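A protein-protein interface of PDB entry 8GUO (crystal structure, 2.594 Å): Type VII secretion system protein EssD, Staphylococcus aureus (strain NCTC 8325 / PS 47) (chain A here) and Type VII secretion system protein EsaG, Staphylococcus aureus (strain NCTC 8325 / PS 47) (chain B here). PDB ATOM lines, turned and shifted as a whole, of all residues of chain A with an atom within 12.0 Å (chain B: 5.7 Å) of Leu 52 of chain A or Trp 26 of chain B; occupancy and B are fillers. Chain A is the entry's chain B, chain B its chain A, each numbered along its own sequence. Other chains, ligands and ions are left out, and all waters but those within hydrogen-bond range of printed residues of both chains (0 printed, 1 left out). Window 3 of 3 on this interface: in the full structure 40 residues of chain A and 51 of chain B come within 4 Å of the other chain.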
ATOM      1  N   HIS A  32       2.276 -23.531  -4.560  1.00  0.00           N
ATOM      2  CA  HIS A  32       2.216 -24.234  -3.287  1.00  0.00           C
ATOM      3  C   HIS A  32       2.401 -25.735  -3.477  1.00  0.00           C
ATOM      4  O   HIS A  32       1.672 -26.355  -4.246  1.00  0.00           O
ATOM      5  CB  HIS A  32       0.877 -23.945  -2.611  1.00  0.00           C
ATOM      6  CG  HIS A  32       0.733 -22.535  -2.134  1.00  0.00           C
ATOM      7  ND1 HIS A  32       0.442 -22.205  -0.828  1.00  0.00           N
ATOM      8  CD2 HIS A  32       0.916 -21.356  -2.781  1.00  0.00           C
ATOM      9  CE1 HIS A  32       0.399 -20.891  -0.703  1.00  0.00           C
ATOM     10  NE2 HIS A  32       0.693 -20.353  -1.872  1.00  0.00           N
ATOM     11  N   VAL A  47       5.535 -23.323   0.987  1.00  0.00           N
ATOM     12  CA  VAL A  47       5.031 -22.030   0.544  1.00  0.00           C
ATOM     13  C   VAL A  47       6.138 -20.983   0.623  1.00  0.00           C
ATOM     14  O   VAL A  47       6.618 -20.667   1.712  1.00  0.00           O
ATOM     15  CB  VAL A  47       3.836 -21.553   1.411  1.00  0.00           C
ATOM     16  CG1 VAL A  47       3.396 -20.158   0.993  1.00  0.00           C
ATOM     17  CG2 VAL A  47       2.679 -22.532   1.354  1.00  0.00           C
ATOM     18  N   ASP A  48       6.550 -20.453  -0.526  1.00  0.00           N
ATOM     19  CA  ASP A  48       7.502 -19.345  -0.551  1.00  0.00           C
ATOM     20  C   ASP A  48       6.775 -18.031  -0.803  1.00  0.00           C
ATOM     21  O   ASP A  48       7.353 -17.083  -1.332  1.00  0.00           O
ATOM     22  CB  ASP A  48       8.577 -19.565  -1.621  1.00  0.00           C
ATOM     23  CG  ASP A  48       8.009 -19.628  -3.037  1.00  0.00           C
ATOM     24  OD1 ASP A  48       6.794 -19.416  -3.238  1.00  0.00           O
ATOM     25  OD2 ASP A  48       8.798 -19.893  -3.966  1.00  0.00           O
ATOM     26  N   ASN A  49       5.508 -17.983  -0.403  1.00  0.00           N
ATOM     27  CA  ASN A  49       4.576 -16.995  -0.930  1.00  0.00           C
ATOM     28  C   ASN A  49       3.805 -16.176   0.114  1.00  0.00           C
ATOM     29  O   ASN A  49       2.977 -15.343  -0.251  1.00  0.00           O
ATOM     30  CB  ASN A  49       3.583 -17.716  -1.849  1.00  0.00           C
ATOM     31  CG  ASN A  49       3.045 -16.828  -2.946  1.00  0.00           C
ATOM     32  OD1 ASN A  49       3.513 -15.706  -3.140  1.00  0.00           O
ATOM     33  ND2 ASN A  49       2.062 -17.332  -3.683  1.00  0.00           N
ATOM     34  N   LEU A  50       4.078 -16.409   1.397  1.00  0.00           N
ATOM     35  CA  LEU A  50       3.386 -15.710   2.486  1.00  0.00           C
ATOM     36  C   LEU A  50       3.398 -14.188   2.345  1.00  0.00           C
ATOM     37  O   LEU A  50       4.443 -13.587   2.093  1.00  0.00           O
ATOM     38  CB  LEU A  50       4.003 -16.075   3.842  1.00  0.00           C
ATOM     39  CG  LEU A  50       3.659 -17.388   4.548  1.00  0.00           C
ATOM     40  CD1 LEU A  50       4.386 -17.465   5.890  1.00  0.00           C
ATOM     41  CD2 LEU A  50       2.163 -17.535   4.747  1.00  0.00           C
ATOM     42  N   SER A  51       2.232 -13.570   2.511  1.00  0.00           N
ATOM     43  CA  SER A  51       2.139 -12.116   2.573  1.00  0.00           C
ATOM     44  C   SER A  51       2.079 -11.665   4.029  1.00  0.00           C
ATOM     45  O   SER A  51       1.077 -11.875   4.710  1.00  0.00           O
ATOM     46  CB  SER A  51       0.915 -11.608   1.807  1.00  0.00           C
ATOM     47  OG  SER A  51      -0.278 -12.188   2.301  1.00  0.00           O
ATOM     48  N   LEU A  52       3.161 -11.052   4.496  1.00  0.00           N
ATOM     49  CA  LEU A  52       3.244 -10.566   5.869  1.00  0.00           C
ATOM     50  C   LEU A  52       3.093  -9.047   5.921  1.00  0.00           C
ATOM     51  O   LEU A  52       2.084  -8.527   6.407  1.00  0.00           O
ATOM     52  CB  LEU A  52       4.569 -10.984   6.507  1.00  0.00           C
ATOM     53  CG  LEU A  52       4.847 -12.483   6.633  1.00  0.00           C
ATOM     54  CD1 LEU A  52       6.334 -12.743   6.794  1.00  0.00           C
ATOM     55  CD2 LEU A  52       4.081 -13.079   7.802  1.00  0.00           C
ATOM     56  N   ASN B  12      -1.770 -17.406   5.988  1.00  0.00           N
ATOM     57  CA  ASN B  12      -1.470 -15.986   6.094  1.00  0.00           C
ATOM     58  C   ASN B  12      -2.019 -15.375   7.378  1.00  0.00           C
ATOM     59  O   ASN B  12      -1.377 -14.528   7.998  1.00  0.00           O
ATOM     60  CB  ASN B  12      -2.031 -15.240   4.878  1.00  0.00           C
ATOM     61  CG  ASN B  12      -1.169 -15.409   3.639  1.00  0.00           C
ATOM     62  OD1 ASN B  12       0.051 -15.269   3.696  1.00  0.00           O
ATOM     63  ND2 ASN B  12      -1.802 -15.715   2.513  1.00  0.00           N
ATOM     64  N   ALA B  15       0.125 -16.741  10.335  1.00  0.00           N
ATOM     65  CA  ALA B  15       1.448 -16.127  10.304  1.00  0.00           C
ATOM     66  C   ALA B  15       1.438 -14.696  10.841  1.00  0.00           C
ATOM     67  O   ALA B  15       2.323 -14.306  11.604  1.00  0.00           O
ATOM     68  CB  ALA B  15       2.000 -16.149   8.890  1.00  0.00           C
ATOM     69  N   ASN B  16       0.435 -13.919  10.439  1.00  0.00           N
ATOM     70  CA  ASN B  16       0.331 -12.519  10.846  1.00  0.00           C
ATOM     71  C   ASN B  16      -0.139 -12.345  12.286  1.00  0.00           C
ATOM     72  O   ASN B  16       0.153 -11.332  12.918  1.00  0.00           O
ATOM     73  CB  ASN B  16      -0.606 -11.756   9.905  1.00  0.00           C
ATOM     74  CG  ASN B  16       0.035 -11.448   8.565  1.00  0.00           C
ATOM     75  OD1 ASN B  16       0.973 -10.655   8.483  1.00  0.00           O
ATOM     76  ND2 ASN B  16      -0.477 -12.064   7.504  1.00  0.00           N
ATOM     77  N   SER B  19       3.026 -13.041  14.326  1.00  0.00           N
ATOM     78  CA  SER B  19       3.938 -11.916  14.144  1.00  0.00           C
ATOM     79  C   SER B  19       3.567 -10.709  15.005  1.00  0.00           C
ATOM     80  O   SER B  19       4.439  -9.963  15.448  1.00  0.00           O
ATOM     81  CB  SER B  19       3.980 -11.514  12.668  1.00  0.00           C
ATOM     82  OG  SER B  19       4.746 -10.339  12.483  1.00  0.00           O
ATOM     83  N   ILE B  22       4.675 -10.943  18.613  1.00  0.00           N
ATOM     84  CA  ILE B  22       6.091 -10.655  18.803  1.00  0.00           C
ATOM     85  C   ILE B  22       6.324  -9.150  18.690  1.00  0.00           C
ATOM     86  O   ILE B  22       6.087  -8.558  17.637  1.00  0.00           O
ATOM     87  CB  ILE B  22       6.962 -11.397  17.774  1.00  0.00           C
ATOM     88  CG1 ILE B  22       6.600 -12.883  17.743  1.00  0.00           C
ATOM     89  CG2 ILE B  22       8.432 -11.211  18.096  1.00  0.00           C
ATOM     90  CD1 ILE B  22       7.288 -13.659  16.639  1.00  0.00           C
ATOM     91  N   VAL B  24       9.083  -7.419  18.872  1.00  0.00           N
ATOM     92  CA  VAL B  24      10.351  -7.026  18.271  1.00  0.00           C
ATOM     93  C   VAL B  24      10.458  -7.613  16.873  1.00  0.00           C
ATOM     94  O   VAL B  24       9.655  -8.461  16.489  1.00  0.00           O
ATOM     95  CB  VAL B  24      11.546  -7.500  19.104  1.00  0.00           C
ATOM     96  CG1 VAL B  24      11.444  -6.956  20.510  1.00  0.00           C
ATOM     97  CG2 VAL B  24      11.600  -9.020  19.120  1.00  0.00           C
ATOM     98  N   GLU B  25      11.448  -7.173  16.108  1.00  0.00           N
ATOM     99  CA  GLU B  25      11.645  -7.764  14.797  1.00  0.00           C
ATOM    100  C   GLU B  25      12.179  -9.181  14.942  1.00  0.00           C
ATOM    101  O   GLU B  25      13.121  -9.435  15.694  1.00  0.00           O
ATOM    102  CB  GLU B  25      12.590  -6.936  13.939  1.00  0.00           C
ATOM    103  CG  GLU B  25      12.961  -7.653  12.659  1.00  0.00           C
ATOM    104  CD  GLU B  25      13.670  -6.764  11.679  1.00  0.00           C
ATOM    105  OE1 GLU B  25      14.036  -7.256  10.591  1.00  0.00           O
ATOM    106  OE2 GLU B  25      13.885  -5.578  12.002  1.00  0.00           O
ATOM    107  N   TRP B  26      11.555 -10.098  14.215  1.00  0.00           N
ATOM    108  CA  TRP B  26      11.922 -11.502  14.250  1.00  0.00           C
ATOM    109  C   TRP B  26      12.403 -11.938  12.873  1.00  0.00           C
ATOM    110  O   TRP B  26      12.151 -11.252  11.884  1.00  0.00           O
ATOM    111  CB  TRP B  26      10.727 -12.342  14.693  1.00  0.00           C
ATOM    112  CG  TRP B  26       9.511 -12.076  13.862  1.00  0.00           C
ATOM    113  CD1 TRP B  26       8.550 -11.132  14.086  1.00  0.00           C
ATOM    114  CD2 TRP B  26       9.137 -12.753  12.659  1.00  0.00           C
ATOM    115  NE1 TRP B  26       7.596 -11.187  13.099  1.00  0.00           N
ATOM    116  CE2 TRP B  26       7.933 -12.174  12.211  1.00  0.00           C
ATOM    117  CE3 TRP B  26       9.700 -13.796  11.922  1.00  0.00           C
ATOM    118  CZ2 TRP B  26       7.285 -12.606  11.057  1.00  0.00           C
ATOM    119  CZ3 TRP B  26       9.057 -14.222  10.780  1.00  0.00           C
ATOM    120  CH2 TRP B  26       7.863 -13.628  10.357  1.00  0.00           C
ATOM    121  N   GLU B  27      13.091 -13.074  12.805  1.00  0.00           N
ATOM    122  CA  GLU B  27      13.545 -13.599  11.522  1.00  0.00           C
ATOM    123  C   GLU B  27      12.823 -14.895  11.164  1.00  0.00           C
ATOM    124  O   GLU B  27      12.313 -15.041  10.055  1.00  0.00           O
ATOM    125  CB  GLU B  27      15.058 -13.822  11.531  1.00  0.00           C
ATOM    126  CG  GLU B  27      15.685 -13.744  10.149  1.00  0.00           C
ATOM    127  CD  GLU B  27      17.149 -14.138  10.133  1.00  0.00           C
ATOM    128  OE1 GLU B  27      17.804 -14.059  11.194  1.00  0.00           O
ATOM    129  OE2 GLU B  27      17.645 -14.523   9.053  1.00  0.00           O
ATOM    130  N   LYS B  28      12.790 -15.839  12.102  1.00  0.00           N
ATOM    131  CA  LYS B  28      12.082 -17.099  11.889  1.00  0.00           C
ATOM    132  C   LYS B  28      11.208 -17.458  13.084  1.00  0.00           C
ATOM    133  O   LYS B  28      11.521 -17.115  14.222  1.00  0.00           O
ATOM    134  CB  LYS B  28      13.069 -18.237  11.608  1.00  0.00           C
ATOM    135  CG  LYS B  28      14.217 -17.873  10.673  1.00  0.00           C
ATOM    136  CD  LYS B  28      15.197 -19.028  10.534  1.00  0.00           C
ATOM    137  CE  LYS B  28      16.318 -18.716   9.551  1.00  0.00           C
ATOM    138  NZ  LYS B  28      17.292 -19.843   9.477  1.00  0.00           N
ATOM    139  N   VAL B  29      10.103 -18.145  12.811  1.00  0.00           N
ATOM    140  CA  VAL B  29       9.210 -18.617  13.857  1.00  0.00           C
ATOM    141  C   VAL B  29       8.918 -20.099  13.677  1.00  0.00           C
ATOM    142  O   VAL B  29       8.459 -20.517  12.619  1.00  0.00           O
ATOM    143  CB  VAL B  29       7.871 -17.846  13.865  1.00  0.00           C
ATOM    144  CG1 VAL B  29       7.019 -18.293  15.043  1.00  0.00           C
ATOM    145  CG2 VAL B  29       8.110 -16.349  13.913  1.00  0.00           C
ATOM    146  N   TYR B  46      10.716 -18.058  18.426  1.00  0.00           N
ATOM    147  CA  TYR B  46      11.149 -17.139  17.379  1.00  0.00           C
ATOM    148  C   TYR B  46      12.613 -16.758  17.538  1.00  0.00           C
ATOM    149  O   TYR B  46      13.150 -16.768  18.645  1.00  0.00           O
ATOM    150  CB  TYR B  46      10.281 -15.875  17.363  1.00  0.00           C
ATOM    151  CG  TYR B  46      10.507 -14.925  18.522  1.00  0.00           C
ATOM    152  CD1 TYR B  46      11.431 -13.889  18.432  1.00  0.00           C
ATOM    153  CD2 TYR B  46       9.778 -15.049  19.693  1.00  0.00           C
ATOM    154  CE1 TYR B  46      11.631 -13.017  19.483  1.00  0.00           C
ATOM    155  CE2 TYR B  46       9.968 -14.179  20.747  1.00  0.00           C
ATOM    156  CZ  TYR B  46      10.897 -13.168  20.637  1.00  0.00           C
ATOM    157  OH  TYR B  46      11.092 -12.303  21.684  1.00  0.00           O
ATOM    158  N   THR B  47      13.251 -16.423  16.421  1.00  0.00           N
ATOM    159  CA  THR B  47      14.621 -15.930  16.437  1.00  0.00           C
ATOM    160  C   THR B  47      14.646 -14.464  16.028  1.00  0.00           C
ATOM    161  O   THR B  47      13.713 -13.974  15.392  1.00  0.00           O
ATOM    162  CB  THR B  47      15.533 -16.734  15.493  1.00  0.00           C
ATOM    163  OG1 THR B  47      15.181 -16.452  14.134  1.00  0.00           O
ATOM    164  CG2 THR B  47      15.399 -18.225  15.753  1.00  0.00           C
ATOM    165  N   LYS B  48      15.712 -13.770  16.408  1.00  0.00           N
ATOM    166  CA  LYS B  48      15.936 -12.398  15.972  1.00  0.00           C
ATOM    167  C   LYS B  48      17.105 -12.377  14.997  1.00  0.00           C
ATOM    168  O   LYS B  48      17.993 -13.222  15.085  1.00  0.00           O
ATOM    169  CB  LYS B  48      16.215 -11.479  17.169  1.00  0.00           C
ATOM    170  CG  LYS B  48      15.269 -11.650  18.342  1.00  0.00           C
ATOM    171  CD  LYS B  48      15.781 -10.888  19.560  1.00  0.00           C
ATOM    172  CE  LYS B  48      14.948 -11.165  20.799  1.00  0.00           C
ATOM    173  NZ  LYS B  48      15.498 -10.455  21.985  1.00  0.00           N
ATOM    174  N   PRO B  49      17.109 -11.414  14.061  1.00  0.00           N
ATOM    175  CA  PRO B  49      18.207 -11.344  13.090  1.00  0.00           C
ATOM    176  C   PRO B  49      19.540 -11.013  13.755  1.00  0.00           C
ATOM    177  O   PRO B  49      19.624 -10.076  14.551  1.00  0.00           O
ATOM    178  CB  PRO B  49      17.766 -10.226  12.142  1.00  0.00           C
ATOM    179  CG  PRO B  49      16.819  -9.398  12.939  1.00  0.00           C
ATOM    180  CD  PRO B  49      16.102 -10.361  13.839  1.00  0.00           C
ATOM    181  N   PHE B 104       7.967 -20.452   9.613  1.00  0.00           N
ATOM    182  CA  PHE B 104       8.072 -19.441   8.575  1.00  0.00           C
ATOM    183  C   PHE B 104       9.137 -18.399   8.867  1.00  0.00           C
ATOM    184  O   PHE B 104       9.512 -18.174  10.017  1.00  0.00           O
ATOM    185  CB  PHE B 104       6.720 -18.753   8.346  1.00  0.00           C
ATOM    186  CG  PHE B 104       6.136 -18.113   9.570  1.00  0.00           C
ATOM    187  CD1 PHE B 104       5.456 -18.876  10.501  1.00  0.00           C
ATOM    188  CD2 PHE B 104       6.235 -16.745   9.775  1.00  0.00           C
ATOM    189  CE1 PHE B 104       4.904 -18.297  11.623  1.00  0.00           C
ATOM    190  CE2 PHE B 104       5.682 -16.159  10.899  1.00  0.00           C
ATOM    191  CZ  PHE B 104       5.015 -16.938  11.822  1.00  0.00           C
ATOM    192  N   THR B 105       9.626 -17.776   7.800  1.00  0.00           N
ATOM    193  CA  THR B 105      10.641 -16.742   7.895  1.00  0.00           C
ATOM    194  C   THR B 105      10.004 -15.404   7.555  1.00  0.00           C
ATOM    195  O   THR B 105       8.907 -15.367   6.998  1.00  0.00           O
ATOM    196  CB  THR B 105      11.823 -17.011   6.946  1.00  0.00           C
ATOM    197  OG1 THR B 105      11.368 -16.961   5.588  1.00  0.00           O
ATOM    198  CG2 THR B 105      12.434 -18.379   7.221  1.00  0.00           C
ATOM    199  N   ARG B 106      10.683 -14.312   7.890  1.00  0.00           N
ATOM    200  CA  ARG B 106      10.176 -12.978   7.586  1.00  0.00           C
ATOM    201  C   ARG B 106      10.210 -12.694   6.088  1.00  0.00           C
ATOM    202  O   ARG B 106       9.505 -11.813   5.600  1.00  0.00           O
ATOM    203  CB  ARG B 106      10.981 -11.918   8.342  1.00  0.00           C
ATOM    204  CG  ARG B 106      12.435 -11.842   7.918  1.00  0.00           C
ATOM    205  CD  ARG B 106      13.153 -10.682   8.569  1.00  0.00           C
ATOM    206  NE  ARG B 106      14.600 -10.833   8.475  1.00  0.00           N
ATOM    207  CZ  ARG B 106      15.470  -9.893   8.825  1.00  0.00           C
ATOM    208  NH1 ARG B 106      16.771 -10.111   8.710  1.00  0.00           N
ATOM    209  NH2 ARG B 106      15.033  -8.734   9.287  1.00  0.00           N
ATOM    210  N   GLU B 107      11.034 -13.444   5.362  1.00  0.00           N
ATOM    211  CA  GLU B 107      11.117 -13.305   3.913  1.00  0.00           C
ATOM    212  C   GLU B 107       9.912 -13.941   3.224  1.00  0.00           C
ATOM    213  O   GLU B 107       9.675 -13.713   2.039  1.00  0.00           O
ATOM    214  CB  GLU B 107      12.414 -13.920   3.377  1.00  0.00           C
ATOM    215  CG  GLU B 107      13.686 -13.222   3.843  1.00  0.00           C
ATOM    216  CD  GLU B 107      14.174 -13.710   5.192  1.00  0.00           C
ATOM    217  OE1 GLU B 107      13.522 -14.594   5.781  1.00  0.00           O
ATOM    218  OE2 GLU B 107      15.215 -13.206   5.665  1.00  0.00           O
ATOM    219  N   GLY B 108       9.155 -14.746   3.963  1.00  0.00           N
ATOM    220  CA  GLY B 108       7.902 -15.265   3.449  1.00  0.00           C
ATOM    221  C   GLY B 108       7.847 -16.761   3.206  1.00  0.00           C
ATOM    222  O   GLY B 108       6.829 -17.273   2.747  1.00  0.00           O
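Among the printed residues, merely in contact across the chains: Val 47 of chain A with Gly 108 of chain B (3.6 Å), Asp 48 of chain A with Gly 108 of chain B (3.6 Å), Leu 50 of chain A with Asn 12 of chain B (3.3 Å), Leu 50 of chain A with Phe 104 of chain B (3.6 Å), Leu 52 of chain A with Ala 15 of chain B (3.9 Å), Leu 52 of chain A with Trp 26 of chain B (3.98 Å), Leu 52 of chain A with Thr 105 of chain B (3.7 Å) and Leu 52 of chain A with Arg 106 of chain B (3.5 Å).
Printed residues of chain B that touch a printed residue of chain A: Asn 12, Ala 15, Asn 16, Trp 26, Phe 104, Thr 105, Arg 106 and Gly 108. Of the 7 printed residues of chain A, 6 touch a printed residue of chain B. Printed residues of chain A that touch a printed residue of chain B: Val 47, Asp 48, Asn 49, Leu 50, Ser 51 and Leu 52. Among the printed residues, 13 pairs touch across the chains. Among the printed residues, no Asp or Glu carboxylate lies within 4 Å of a Lys or Arg side-chain nitrogen of the other chain.
Leu 52 of chain A touches just these residues of chain B: Ala 15 (3.9 Å), Asn 16 (3.2 Å), Trp 26 (3.98 Å), Thr 105 (3.7 Å) and Arg 106 (3.5 Å). Of chain A, only Leu 52 comes within 4 Å of Trp 26 of chain B. Asn 12 of chain B touches just these residues of chain A: Leu 50 and Ser 51. Of chain A, only Leu 52 comes within 4 Å of Ala 15 of chain B. Of chain A, only Ser 51 (3.2 Å) and Leu 52 (3.2 Å) come within 4 Å of Asn 16 of chain B. No residue of chain A comes within 4 Å of Ser 19 of chain B. No residue of chain A comes within 4 Å of Ile 22 of chain B. No residue of chain A comes within 4 Å of Glu 25 of chain B. No residue of chain A comes within 4 Å of Val 29 of chain B. No residue of chain A comes within 4 Å of Tyr 46 of chain B. Thr 47 of chain B touches none of the printed residues of chain A. No residue of chain A comes within 4 Å of Pro 49 of chain B. Of the printed residues of chain A, Thr 105 of chain B touches Leu 52. Arg 106 of chain B touches just one residue of chain A: Leu 52. No residue of chain A comes within 4 Å of Glu 107 of chain B. Printed residues of chain B within 4 Å of Val 47 of chain A: Gly 108. Printed residues of chain B within 4 Å of Asp 48 of chain A: Gly 108. Lys 48 of chain B touches none of the printed residues of chain A. The nearest residue of chain A that does not touch Trp 26 of chain B is Leu 50 of chain A (6.8 Å). The nearest printed residue of chain B that does not touch Asp 48 of chain A is Glu 107 of chain B (5.3 Å).
The backbone NH (N) of Val 29 of chain B is in hydrogen-bond range of the backbone carbonyl oxygen (O) of Phe 104 of chain B (2.9 Å). The side-chain hydroxyl (OG) of Ser 19 of chain B sits at hydrogen-bond distance from the indole nitrogen (NE1) of Trp 26 of chain B, at 3.0 Å. The guanidinium group (NE) of Arg 106 of chain B lies within salt-bridge range of the side-chain carboxylate (OE2) of Glu 107 of chain B, 3.7 Å away. The side-chain amide nitrogen (ND2) of Asn 16 of chain B is in hydrogen-bond range of the backbone carbonyl oxygen (O) of Asn 12 of chain B (2.7 Å). N of Arg 106 of chain B is in hydrogen-bond range of O of Glu 27 of chain B (2.8 Å). The side-chain hydroxyl (OG1) of Thr 105 of chain B sits close to the side-chain carboxylate (OE1) of Glu 107 of chain B (3.2 Å).
The backbone carbonyl oxygen (O) of Gly 108 of chain B lies within hydrogen-bond range of the backbone NH (N) of Leu 50 of chain A (3.2 Å). OD1 of Asn 16 of chain B lies close to O of Leu 52 of chain A (3.2 Å). The side-chain amide oxygen (OD1) of Asn 12 of chain B is in hydrogen-bond range of the backbone NH (N) of Ser 51 of chain A. The side-chain amide nitrogen (ND2) of Asn 16 of chain B is in hydrogen-bond range of the backbone carbonyl oxygen (O) of Ser 51 of chain A (3.2 Å). The backbone carbonyl oxygen of Gly 108 of chain B sits at hydrogen-bond distance from the backbone NH of Asn 49 of chain A (3.5 Å).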
